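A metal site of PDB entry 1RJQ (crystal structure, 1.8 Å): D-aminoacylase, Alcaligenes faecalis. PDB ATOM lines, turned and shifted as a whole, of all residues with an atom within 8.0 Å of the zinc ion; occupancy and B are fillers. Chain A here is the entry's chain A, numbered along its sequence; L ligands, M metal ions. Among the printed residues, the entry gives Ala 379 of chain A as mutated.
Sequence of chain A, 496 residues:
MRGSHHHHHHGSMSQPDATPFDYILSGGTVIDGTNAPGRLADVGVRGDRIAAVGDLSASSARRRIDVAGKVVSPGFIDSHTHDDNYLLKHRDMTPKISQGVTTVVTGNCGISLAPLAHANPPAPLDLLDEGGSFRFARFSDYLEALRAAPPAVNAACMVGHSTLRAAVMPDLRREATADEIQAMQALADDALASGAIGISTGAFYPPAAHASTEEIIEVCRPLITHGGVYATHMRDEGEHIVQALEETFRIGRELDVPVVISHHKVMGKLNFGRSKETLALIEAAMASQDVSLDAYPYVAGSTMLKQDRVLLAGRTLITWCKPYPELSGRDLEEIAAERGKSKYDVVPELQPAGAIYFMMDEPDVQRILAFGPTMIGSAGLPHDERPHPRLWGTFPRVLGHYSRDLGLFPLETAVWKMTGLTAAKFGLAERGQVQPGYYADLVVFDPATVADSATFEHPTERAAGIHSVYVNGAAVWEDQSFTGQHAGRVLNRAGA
ND1 of His 263 is in hydrogen-bond range of OE2 of Glu 237 (3.2 Å). The backbone NH of Gly 202 lies close to the backbone carbonyl oxygen of Cys 109, 3.4 Å away. OH of Tyr 205 is in hydrogen-bond range of OG1 of Thr 303 (2.8 Å). The backbone carbonyl oxygen (O) of His 263 is in hydrogen-bond range of the side-chain amino group (NZ) of Lys 265 (2.9 Å). The backbone NH (N) of His 233 lies within hydrogen-bond range of the backbone carbonyl oxygen (O) of Thr 201. The side-chain sulfur (SG) of Cys 109 sits close to a ring nitrogen (NE2) of His 80 (3.3 Å).
Tyr 205 touches the zinc ion (OH to ZN, 3.98 Å).
The zinc ion is bound by O1 of the ligand (2.0 Å), ND1 of His 233 (2.0 Å), NE2 of His 263 (2.1 Å) and SG of Cys 109 (2.2 Å). The zinc ion has four donor atoms within binding distance. Slightly farther from the zinc ion lies an oxygen (O2) of the ligand (2.8 Å).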
ATOM      1  N   HIS A  80       3.561 -18.603   3.488  1.00  0.00           N
ATOM      2  CA  HIS A  80       2.244 -18.093   3.830  1.00  0.00           C
ATOM      3  C   HIS A  80       2.233 -17.228   5.079  1.00  0.00           C
ATOM      4  O   HIS A  80       2.059 -17.739   6.182  1.00  0.00           O
ATOM      5  CB  HIS A  80       1.271 -19.249   4.012  1.00  0.00           C
ATOM      6  CG  HIS A  80      -0.165 -18.817   4.052  1.00  0.00           C
ATOM      7  ND1 HIS A  80      -0.957 -18.766   2.930  1.00  0.00           N
ATOM      8  CD2 HIS A  80      -0.933 -18.371   5.077  1.00  0.00           C
ATOM      9  CE1 HIS A  80      -2.149 -18.299   3.255  1.00  0.00           C
ATOM     10  NE2 HIS A  80      -2.159 -18.045   4.551  1.00  0.00           N
ATOM     11  N   HIS A  82       1.088 -13.279   7.052  1.00  0.00           N
ATOM     12  CA  HIS A  82       0.154 -12.168   7.125  1.00  0.00           C
ATOM     13  C   HIS A  82       0.999 -11.109   7.818  1.00  0.00           C
ATOM     14  O   HIS A  82       0.542 -10.446   8.749  1.00  0.00           O
ATOM     15  CB  HIS A  82      -1.069 -12.537   7.971  1.00  0.00           C
ATOM     16  CG  HIS A  82      -1.915 -13.601   7.359  1.00  0.00           C
ATOM     17  ND1 HIS A  82      -2.612 -13.415   6.190  1.00  0.00           N
ATOM     18  CD2 HIS A  82      -2.126 -14.881   7.720  1.00  0.00           C
ATOM     19  CE1 HIS A  82      -3.224 -14.537   5.854  1.00  0.00           C
ATOM     20  NE2 HIS A  82      -2.942 -15.451   6.764  1.00  0.00           N
ATOM     21  N   ASN A 108      -1.755 -12.672   1.776  1.00  0.00           N
ATOM     22  CA  ASN A 108      -2.410 -13.952   1.503  1.00  0.00           C
ATOM     23  C   ASN A 108      -3.895 -13.980   1.840  1.00  0.00           C
ATOM     24  O   ASN A 108      -4.397 -13.133   2.585  1.00  0.00           O
ATOM     25  CB  ASN A 108      -1.709 -15.072   2.270  1.00  0.00           C
ATOM     26  CG  ASN A 108      -0.347 -15.397   1.688  1.00  0.00           C
ATOM     27  OD1 ASN A 108       0.698 -14.960   2.215  1.00  0.00           O
ATOM     28  ND2 ASN A 108      -0.342 -16.131   0.597  1.00  0.00           N
ATOM     29  N   CYS A 109      -4.576 -14.976   1.276  1.00  0.00           N
ATOM     30  CA  CYS A 109      -5.997 -15.203   1.509  1.00  0.00           C
ATOM     31  C   CYS A 109      -6.868 -14.002   1.151  1.00  0.00           C
ATOM     32  O   CYS A 109      -7.943 -13.817   1.727  1.00  0.00           O
ATOM     33  CB  CYS A 109      -6.211 -15.579   2.977  1.00  0.00           C
ATOM     34  SG  CYS A 109      -5.103 -16.887   3.525  1.00  0.00           S
ATOM     35  N   GLY A 110      -6.410 -13.210   0.186  1.00  0.00           N
ATOM     36  CA  GLY A 110      -7.161 -12.044  -0.247  1.00  0.00           C
ATOM     37  C   GLY A 110      -6.980 -10.858   0.686  1.00  0.00           C
ATOM     38  O   GLY A 110      -7.586  -9.798   0.482  1.00  0.00           O
ATOM     39  N   ILE A 111      -6.144 -11.041   1.700  1.00  0.00           N
ATOM     40  CA  ILE A 111      -5.893 -10.017   2.709  1.00  0.00           C
ATOM     41  C   ILE A 111      -4.525  -9.335   2.573  1.00  0.00           C
ATOM     42  O   ILE A 111      -3.501  -9.902   2.951  1.00  0.00           O
ATOM     43  CB  ILE A 111      -5.946 -10.636   4.129  1.00  0.00           C
ATOM     44  CG1 ILE A 111      -7.244 -11.417   4.316  1.00  0.00           C
ATOM     45  CG2 ILE A 111      -5.847  -9.533   5.191  1.00  0.00           C
ATOM     46  CD1 ILE A 111      -7.288 -12.225   5.595  1.00  0.00           C
ATOM     47  N   PRO A 124     -11.776 -10.371   7.632  1.00  0.00           N
ATOM     48  CA  PRO A 124     -10.557 -10.539   8.438  1.00  0.00           C
ATOM     49  C   PRO A 124      -9.398  -9.571   8.141  1.00  0.00           C
ATOM     50  O   PRO A 124      -8.261  -9.843   8.534  1.00  0.00           O
ATOM     51  CB  PRO A 124     -10.167 -11.984   8.131  1.00  0.00           C
ATOM     52  CG  PRO A 124     -10.465 -12.062   6.661  1.00  0.00           C
ATOM     53  CD  PRO A 124     -11.824 -11.377   6.559  1.00  0.00           C
ATOM     54  N   LEU A 127      -7.091  -8.362  10.940  1.00  0.00           N
ATOM     55  CA  LEU A 127      -6.014  -9.173  11.497  1.00  0.00           C
ATOM     56  C   LEU A 127      -4.644  -8.503  11.295  1.00  0.00           C
ATOM     57  O   LEU A 127      -3.687  -8.823  11.995  1.00  0.00           O
ATOM     58  CB  LEU A 127      -6.006 -10.567  10.858  1.00  0.00           C
ATOM     59  CG  LEU A 127      -7.169 -11.494  11.213  1.00  0.00           C
ATOM     60  CD1 LEU A 127      -7.062 -12.776  10.396  1.00  0.00           C
ATOM     61  CD2 LEU A 127      -7.155 -11.807  12.711  1.00  0.00           C
ATOM     62  N   THR A 201      -6.728 -14.599  -3.099  1.00  0.00           N
ATOM     63  CA  THR A 201      -8.154 -14.507  -2.842  1.00  0.00           C
ATOM     64  C   THR A 201      -8.493 -15.328  -1.600  1.00  0.00           C
ATOM     65  O   THR A 201      -7.714 -16.203  -1.194  1.00  0.00           O
ATOM     66  CB  THR A 201      -9.000 -15.089  -3.995  1.00  0.00           C
ATOM     67  OG1 THR A 201      -8.708 -16.483  -4.139  1.00  0.00           O
ATOM     68  CG2 THR A 201      -8.688 -14.368  -5.292  1.00  0.00           C
ATOM     69  N   GLY A 202      -9.642 -15.038  -1.001  1.00  0.00           N
ATOM     70  CA  GLY A 202     -10.098 -15.760   0.173  1.00  0.00           C
ATOM     71  C   GLY A 202     -11.614 -15.663   0.198  1.00  0.00           C
ATOM     72  O   GLY A 202     -12.180 -15.007   1.064  1.00  0.00           O
ATOM     73  N   PHE A 204     -13.640 -17.583   1.130  1.00  0.00           N
ATOM     74  CA  PHE A 204     -14.179 -18.222   2.323  1.00  0.00           C
ATOM     75  C   PHE A 204     -14.664 -17.120   3.279  1.00  0.00           C
ATOM     76  O   PHE A 204     -15.642 -17.305   4.014  1.00  0.00           O
ATOM     77  CB  PHE A 204     -13.087 -19.035   3.016  1.00  0.00           C
ATOM     78  CG  PHE A 204     -13.430 -19.468   4.418  1.00  0.00           C
ATOM     79  CD1 PHE A 204     -14.348 -20.494   4.645  1.00  0.00           C
ATOM     80  CD2 PHE A 204     -12.843 -18.830   5.514  1.00  0.00           C
ATOM     81  CE1 PHE A 204     -14.673 -20.885   5.945  1.00  0.00           C
ATOM     82  CE2 PHE A 204     -13.161 -19.216   6.820  1.00  0.00           C
ATOM     83  CZ  PHE A 204     -14.076 -20.249   7.031  1.00  0.00           C
ATOM     84  N   TYR A 205     -13.976 -15.985   3.264  1.00  0.00           N
ATOM     85  CA  TYR A 205     -14.302 -14.882   4.156  1.00  0.00           C
ATOM     86  C   TYR A 205     -15.422 -13.963   3.693  1.00  0.00           C
ATOM     87  O   TYR A 205     -15.687 -13.812   2.498  1.00  0.00           O
ATOM     88  CB  TYR A 205     -13.022 -14.083   4.441  1.00  0.00           C
ATOM     89  CG  TYR A 205     -11.983 -14.878   5.199  1.00  0.00           C
ATOM     90  CD1 TYR A 205     -12.211 -15.317   6.504  1.00  0.00           C
ATOM     91  CD2 TYR A 205     -10.743 -15.168   4.619  1.00  0.00           C
ATOM     92  CE1 TYR A 205     -11.245 -16.030   7.212  1.00  0.00           C
ATOM     93  CE2 TYR A 205      -9.770 -15.871   5.310  1.00  0.00           C
ATOM     94  CZ  TYR A 205     -10.026 -16.295   6.614  1.00  0.00           C
ATOM     95  OH  TYR A 205      -9.061 -16.979   7.314  1.00  0.00           O
ATOM     96  N   THR A 232      -4.501 -18.832  -3.154  1.00  0.00           N
ATOM     97  CA  THR A 232      -5.859 -18.875  -2.637  1.00  0.00           C
ATOM     98  C   THR A 232      -6.183 -19.644  -1.372  1.00  0.00           C
ATOM     99  O   THR A 232      -5.691 -20.741  -1.121  1.00  0.00           O
ATOM    100  CB  THR A 232      -6.823 -19.401  -3.739  1.00  0.00           C
ATOM    101  OG1 THR A 232      -8.151 -19.518  -3.206  1.00  0.00           O
ATOM    102  CG2 THR A 232      -6.370 -20.787  -4.220  1.00  0.00           C
ATOM    103  N   HIS A 233      -7.026 -19.011  -0.556  1.00  0.00           N
ATOM    104  CA  HIS A 233      -7.570 -19.625   0.637  1.00  0.00           C
ATOM    105  C   HIS A 233      -8.875 -20.065  -0.017  1.00  0.00           C
ATOM    106  O   HIS A 233      -9.776 -19.256  -0.225  1.00  0.00           O
ATOM    107  CB  HIS A 233      -7.824 -18.581   1.725  1.00  0.00           C
ATOM    108  CG  HIS A 233      -8.532 -19.118   2.929  1.00  0.00           C
ATOM    109  ND1 HIS A 233      -8.200 -18.749   4.216  1.00  0.00           N
ATOM    110  CD2 HIS A 233      -9.557 -19.997   3.047  1.00  0.00           C
ATOM    111  CE1 HIS A 233      -8.990 -19.374   5.066  1.00  0.00           C
ATOM    112  NE2 HIS A 233      -9.830 -20.129   4.380  1.00  0.00           N
ATOM    113  N   MET A 234      -8.972 -21.343  -0.360  1.00  0.00           N
ATOM    114  CA  MET A 234     -10.142 -21.852  -1.055  1.00  0.00           C
ATOM    115  C   MET A 234     -11.480 -21.502  -0.415  1.00  0.00           C
ATOM    116  O   MET A 234     -11.573 -21.284   0.796  1.00  0.00           O
ATOM    117  CB  MET A 234      -9.999 -23.365  -1.271  1.00  0.00           C
ATOM    118  CG  MET A 234      -8.730 -23.694  -2.055  1.00  0.00           C
ATOM    119  SD  MET A 234      -8.633 -25.391  -2.668  1.00  0.00           S
ATOM    120  CE  MET A 234      -8.395 -26.280  -1.110  1.00  0.00           C
ATOM    121  N   GLU A 237     -13.008 -25.512   2.885  1.00  0.00           N
ATOM    122  CA  GLU A 237     -11.976 -26.517   3.147  1.00  0.00           C
ATOM    123  C   GLU A 237     -12.537 -27.708   3.908  1.00  0.00           C
ATOM    124  O   GLU A 237     -11.777 -28.455   4.548  1.00  0.00           O
ATOM    125  CB  GLU A 237     -10.826 -25.891   3.938  1.00  0.00           C
ATOM    126  CG  GLU A 237     -10.067 -24.800   3.165  1.00  0.00           C
ATOM    127  CD  GLU A 237      -8.872 -24.282   3.933  1.00  0.00           C
ATOM    128  OE1 GLU A 237      -9.056 -23.777   5.061  1.00  0.00           O
ATOM    129  OE2 GLU A 237      -7.737 -24.389   3.410  1.00  0.00           O
ATOM    130  N   SER A 262      -3.402 -22.331  -0.507  1.00  0.00           N
ATOM    131  CA  SER A 262      -2.932 -21.962   0.816  1.00  0.00           C
ATOM    132  C   SER A 262      -3.354 -22.910   1.932  1.00  0.00           C
ATOM    133  O   SER A 262      -4.442 -23.496   1.871  1.00  0.00           O
ATOM    134  CB  SER A 262      -3.410 -20.542   1.163  1.00  0.00           C
ATOM    135  OG  SER A 262      -2.992 -19.617   0.189  1.00  0.00           O
ATOM    136  N   HIS A 263      -2.495 -23.039   2.937  1.00  0.00           N
ATOM    137  CA  HIS A 263      -2.713 -23.895   4.103  1.00  0.00           C
ATOM    138  C   HIS A 263      -3.699 -25.025   3.862  1.00  0.00           C
ATOM    139  O   HIS A 263      -4.772 -25.074   4.463  1.00  0.00           O
ATOM    140  CB  HIS A 263      -3.170 -23.034   5.304  1.00  0.00           C
ATOM    141  CG  HIS A 263      -4.243 -22.029   4.980  1.00  0.00           C
ATOM    142  ND1 HIS A 263      -5.431 -22.381   4.393  1.00  0.00           N
ATOM    143  CD2 HIS A 263      -4.306 -20.697   5.204  1.00  0.00           C
ATOM    144  CE1 HIS A 263      -6.189 -21.305   4.266  1.00  0.00           C
ATOM    145  NE2 HIS A 263      -5.532 -20.271   4.747  1.00  0.00           N
ATOM    146  N   LYS A 265      -5.781 -28.296   4.002  1.00  0.00           N
ATOM    147  CA  LYS A 265      -6.275 -29.063   5.137  1.00  0.00           C
ATOM    148  C   LYS A 265      -7.658 -29.602   4.772  1.00  0.00           C
ATOM    149  O   LYS A 265      -8.211 -29.274   3.735  1.00  0.00           O
ATOM    150  CB  LYS A 265      -6.467 -28.140   6.344  1.00  0.00           C
ATOM    151  CG  LYS A 265      -7.606 -27.119   6.103  1.00  0.00           C
ATOM    152  CD  LYS A 265      -7.928 -26.246   7.333  1.00  0.00           C
ATOM    153  CE  LYS A 265      -6.829 -25.227   7.622  1.00  0.00           C
ATOM    154  NZ  LYS A 265      -6.686 -24.220   6.528  1.00  0.00           N
ATOM    155  N   TYR A 296       0.760 -25.568   7.267  1.00  0.00           N
ATOM    156  CA  TYR A 296       1.464 -25.367   8.527  1.00  0.00           C
ATOM    157  C   TYR A 296       1.364 -26.687   9.301  1.00  0.00           C
ATOM    158  O   TYR A 296       0.409 -27.447   9.137  1.00  0.00           O
ATOM    159  CB  TYR A 296       0.884 -24.194   9.323  1.00  0.00           C
ATOM    160  CG  TYR A 296      -0.614 -24.194   9.479  1.00  0.00           C
ATOM    161  CD1 TYR A 296      -1.232 -24.987  10.436  1.00  0.00           C
ATOM    162  CD2 TYR A 296      -1.402 -23.368   8.682  1.00  0.00           C
ATOM    163  CE1 TYR A 296      -2.611 -24.956  10.603  1.00  0.00           C
ATOM    164  CE2 TYR A 296      -2.785 -23.338   8.835  1.00  0.00           C
ATOM    165  CZ  TYR A 296      -3.383 -24.127   9.801  1.00  0.00           C
ATOM    166  OH  TYR A 296      -4.740 -24.072   9.954  1.00  0.00           O
ATOM    167  N   SER A 302      -6.457 -20.736  12.797  1.00  0.00           N
ATOM    168  CA  SER A 302      -6.631 -19.466  13.501  1.00  0.00           C
ATOM    169  C   SER A 302      -6.924 -18.358  12.506  1.00  0.00           C
ATOM    170  O   SER A 302      -6.297 -18.265  11.452  1.00  0.00           O
ATOM    171  CB  SER A 302      -5.363 -19.126  14.301  1.00  0.00           C
ATOM    172  OG  SER A 302      -5.540 -17.943  15.061  1.00  0.00           O
ATOM    173  N   THR A 303      -7.890 -17.525  12.842  1.00  0.00           N
ATOM    174  CA  THR A 303      -8.277 -16.403  12.004  1.00  0.00           C
ATOM    175  C   THR A 303      -9.313 -15.594  12.770  1.00  0.00           C
ATOM    176  O   THR A 303      -9.395 -15.681  13.991  1.00  0.00           O
ATOM    177  CB  THR A 303      -8.855 -16.887  10.649  1.00  0.00           C
ATOM    178  OG1 THR A 303      -9.161 -15.758   9.818  1.00  0.00           O
ATOM    179  CG2 THR A 303     -10.120 -17.712  10.858  1.00  0.00           C
ATOM    180  N   ALA A 379       1.334 -19.117   8.366  1.00  0.00           N
ATOM    181  CA  ALA A 379       0.020 -18.518   8.520  1.00  0.00           C
ATOM    182  C   ALA A 379      -0.001 -17.801   9.874  1.00  0.00           C
ATOM    183  O   ALA A 379      -1.048 -17.662  10.518  1.00  0.00           O
ATOM    184  CB  ALA A 379      -1.077 -19.588   8.468  1.00  0.00           C
ATOM    185  N   LEU A 381      -0.204 -15.041  12.706  1.00  0.00           N
ATOM    186  CA  LEU A 381      -0.989 -13.810  12.851  1.00  0.00           C
ATOM    187  C   LEU A 381      -0.248 -13.048  13.951  1.00  0.00           C
ATOM    188  O   LEU A 381      -0.604 -13.128  15.129  1.00  0.00           O
ATOM    189  CB  LEU A 381      -2.429 -14.155  13.263  1.00  0.00           C
ATOM    190  CG  LEU A 381      -3.162 -14.990  12.207  1.00  0.00           C
ATOM    191  CD1 LEU A 381      -4.544 -15.383  12.708  1.00  0.00           C
ATOM    192  CD2 LEU A 381      -3.264 -14.198  10.917  1.00  0.00           C
ATOM    193  N   ARG A 390       2.046 -21.313  15.798  1.00  0.00           N
ATOM    194  CA  ARG A 390       2.637 -21.466  14.472  1.00  0.00           C
ATOM    195  C   ARG A 390       3.412 -20.196  14.119  1.00  0.00           C
ATOM    196  O   ARG A 390       4.370 -20.222  13.340  1.00  0.00           O
ATOM    197  CB  ARG A 390       1.540 -21.739  13.432  1.00  0.00           C
ATOM    198  CG  ARG A 390       0.520 -20.621  13.227  1.00  0.00           C
ATOM    199  CD  ARG A 390      -0.699 -21.156  12.488  1.00  0.00           C
ATOM    200  NE  ARG A 390      -1.583 -20.088  12.036  1.00  0.00           N
ATOM    201  CZ  ARG A 390      -2.803 -20.268  11.560  1.00  0.00           C
ATOM    202  NH1 ARG A 390      -3.305 -21.496  11.478  1.00  0.00           N
ATOM    203  NH2 ARG A 390      -3.520 -19.228  11.138  1.00  0.00           N
HETATM  204  C1  LIG L   1      -5.710 -17.400   7.267  1.00  0.00           C
HETATM  205  O1  LIG L   1      -6.714 -17.491   6.531  1.00  0.00           O
HETATM  206  O2  LIG L   1      -4.591 -17.856   6.947  1.00  0.00           O
HETATM  207  C2  LIG L   1      -5.810 -16.602   8.543  1.00  0.00           C
HETATM  208 ZN    ZN M   1      -6.283 -18.294   4.778  1.00  0.00          ZN
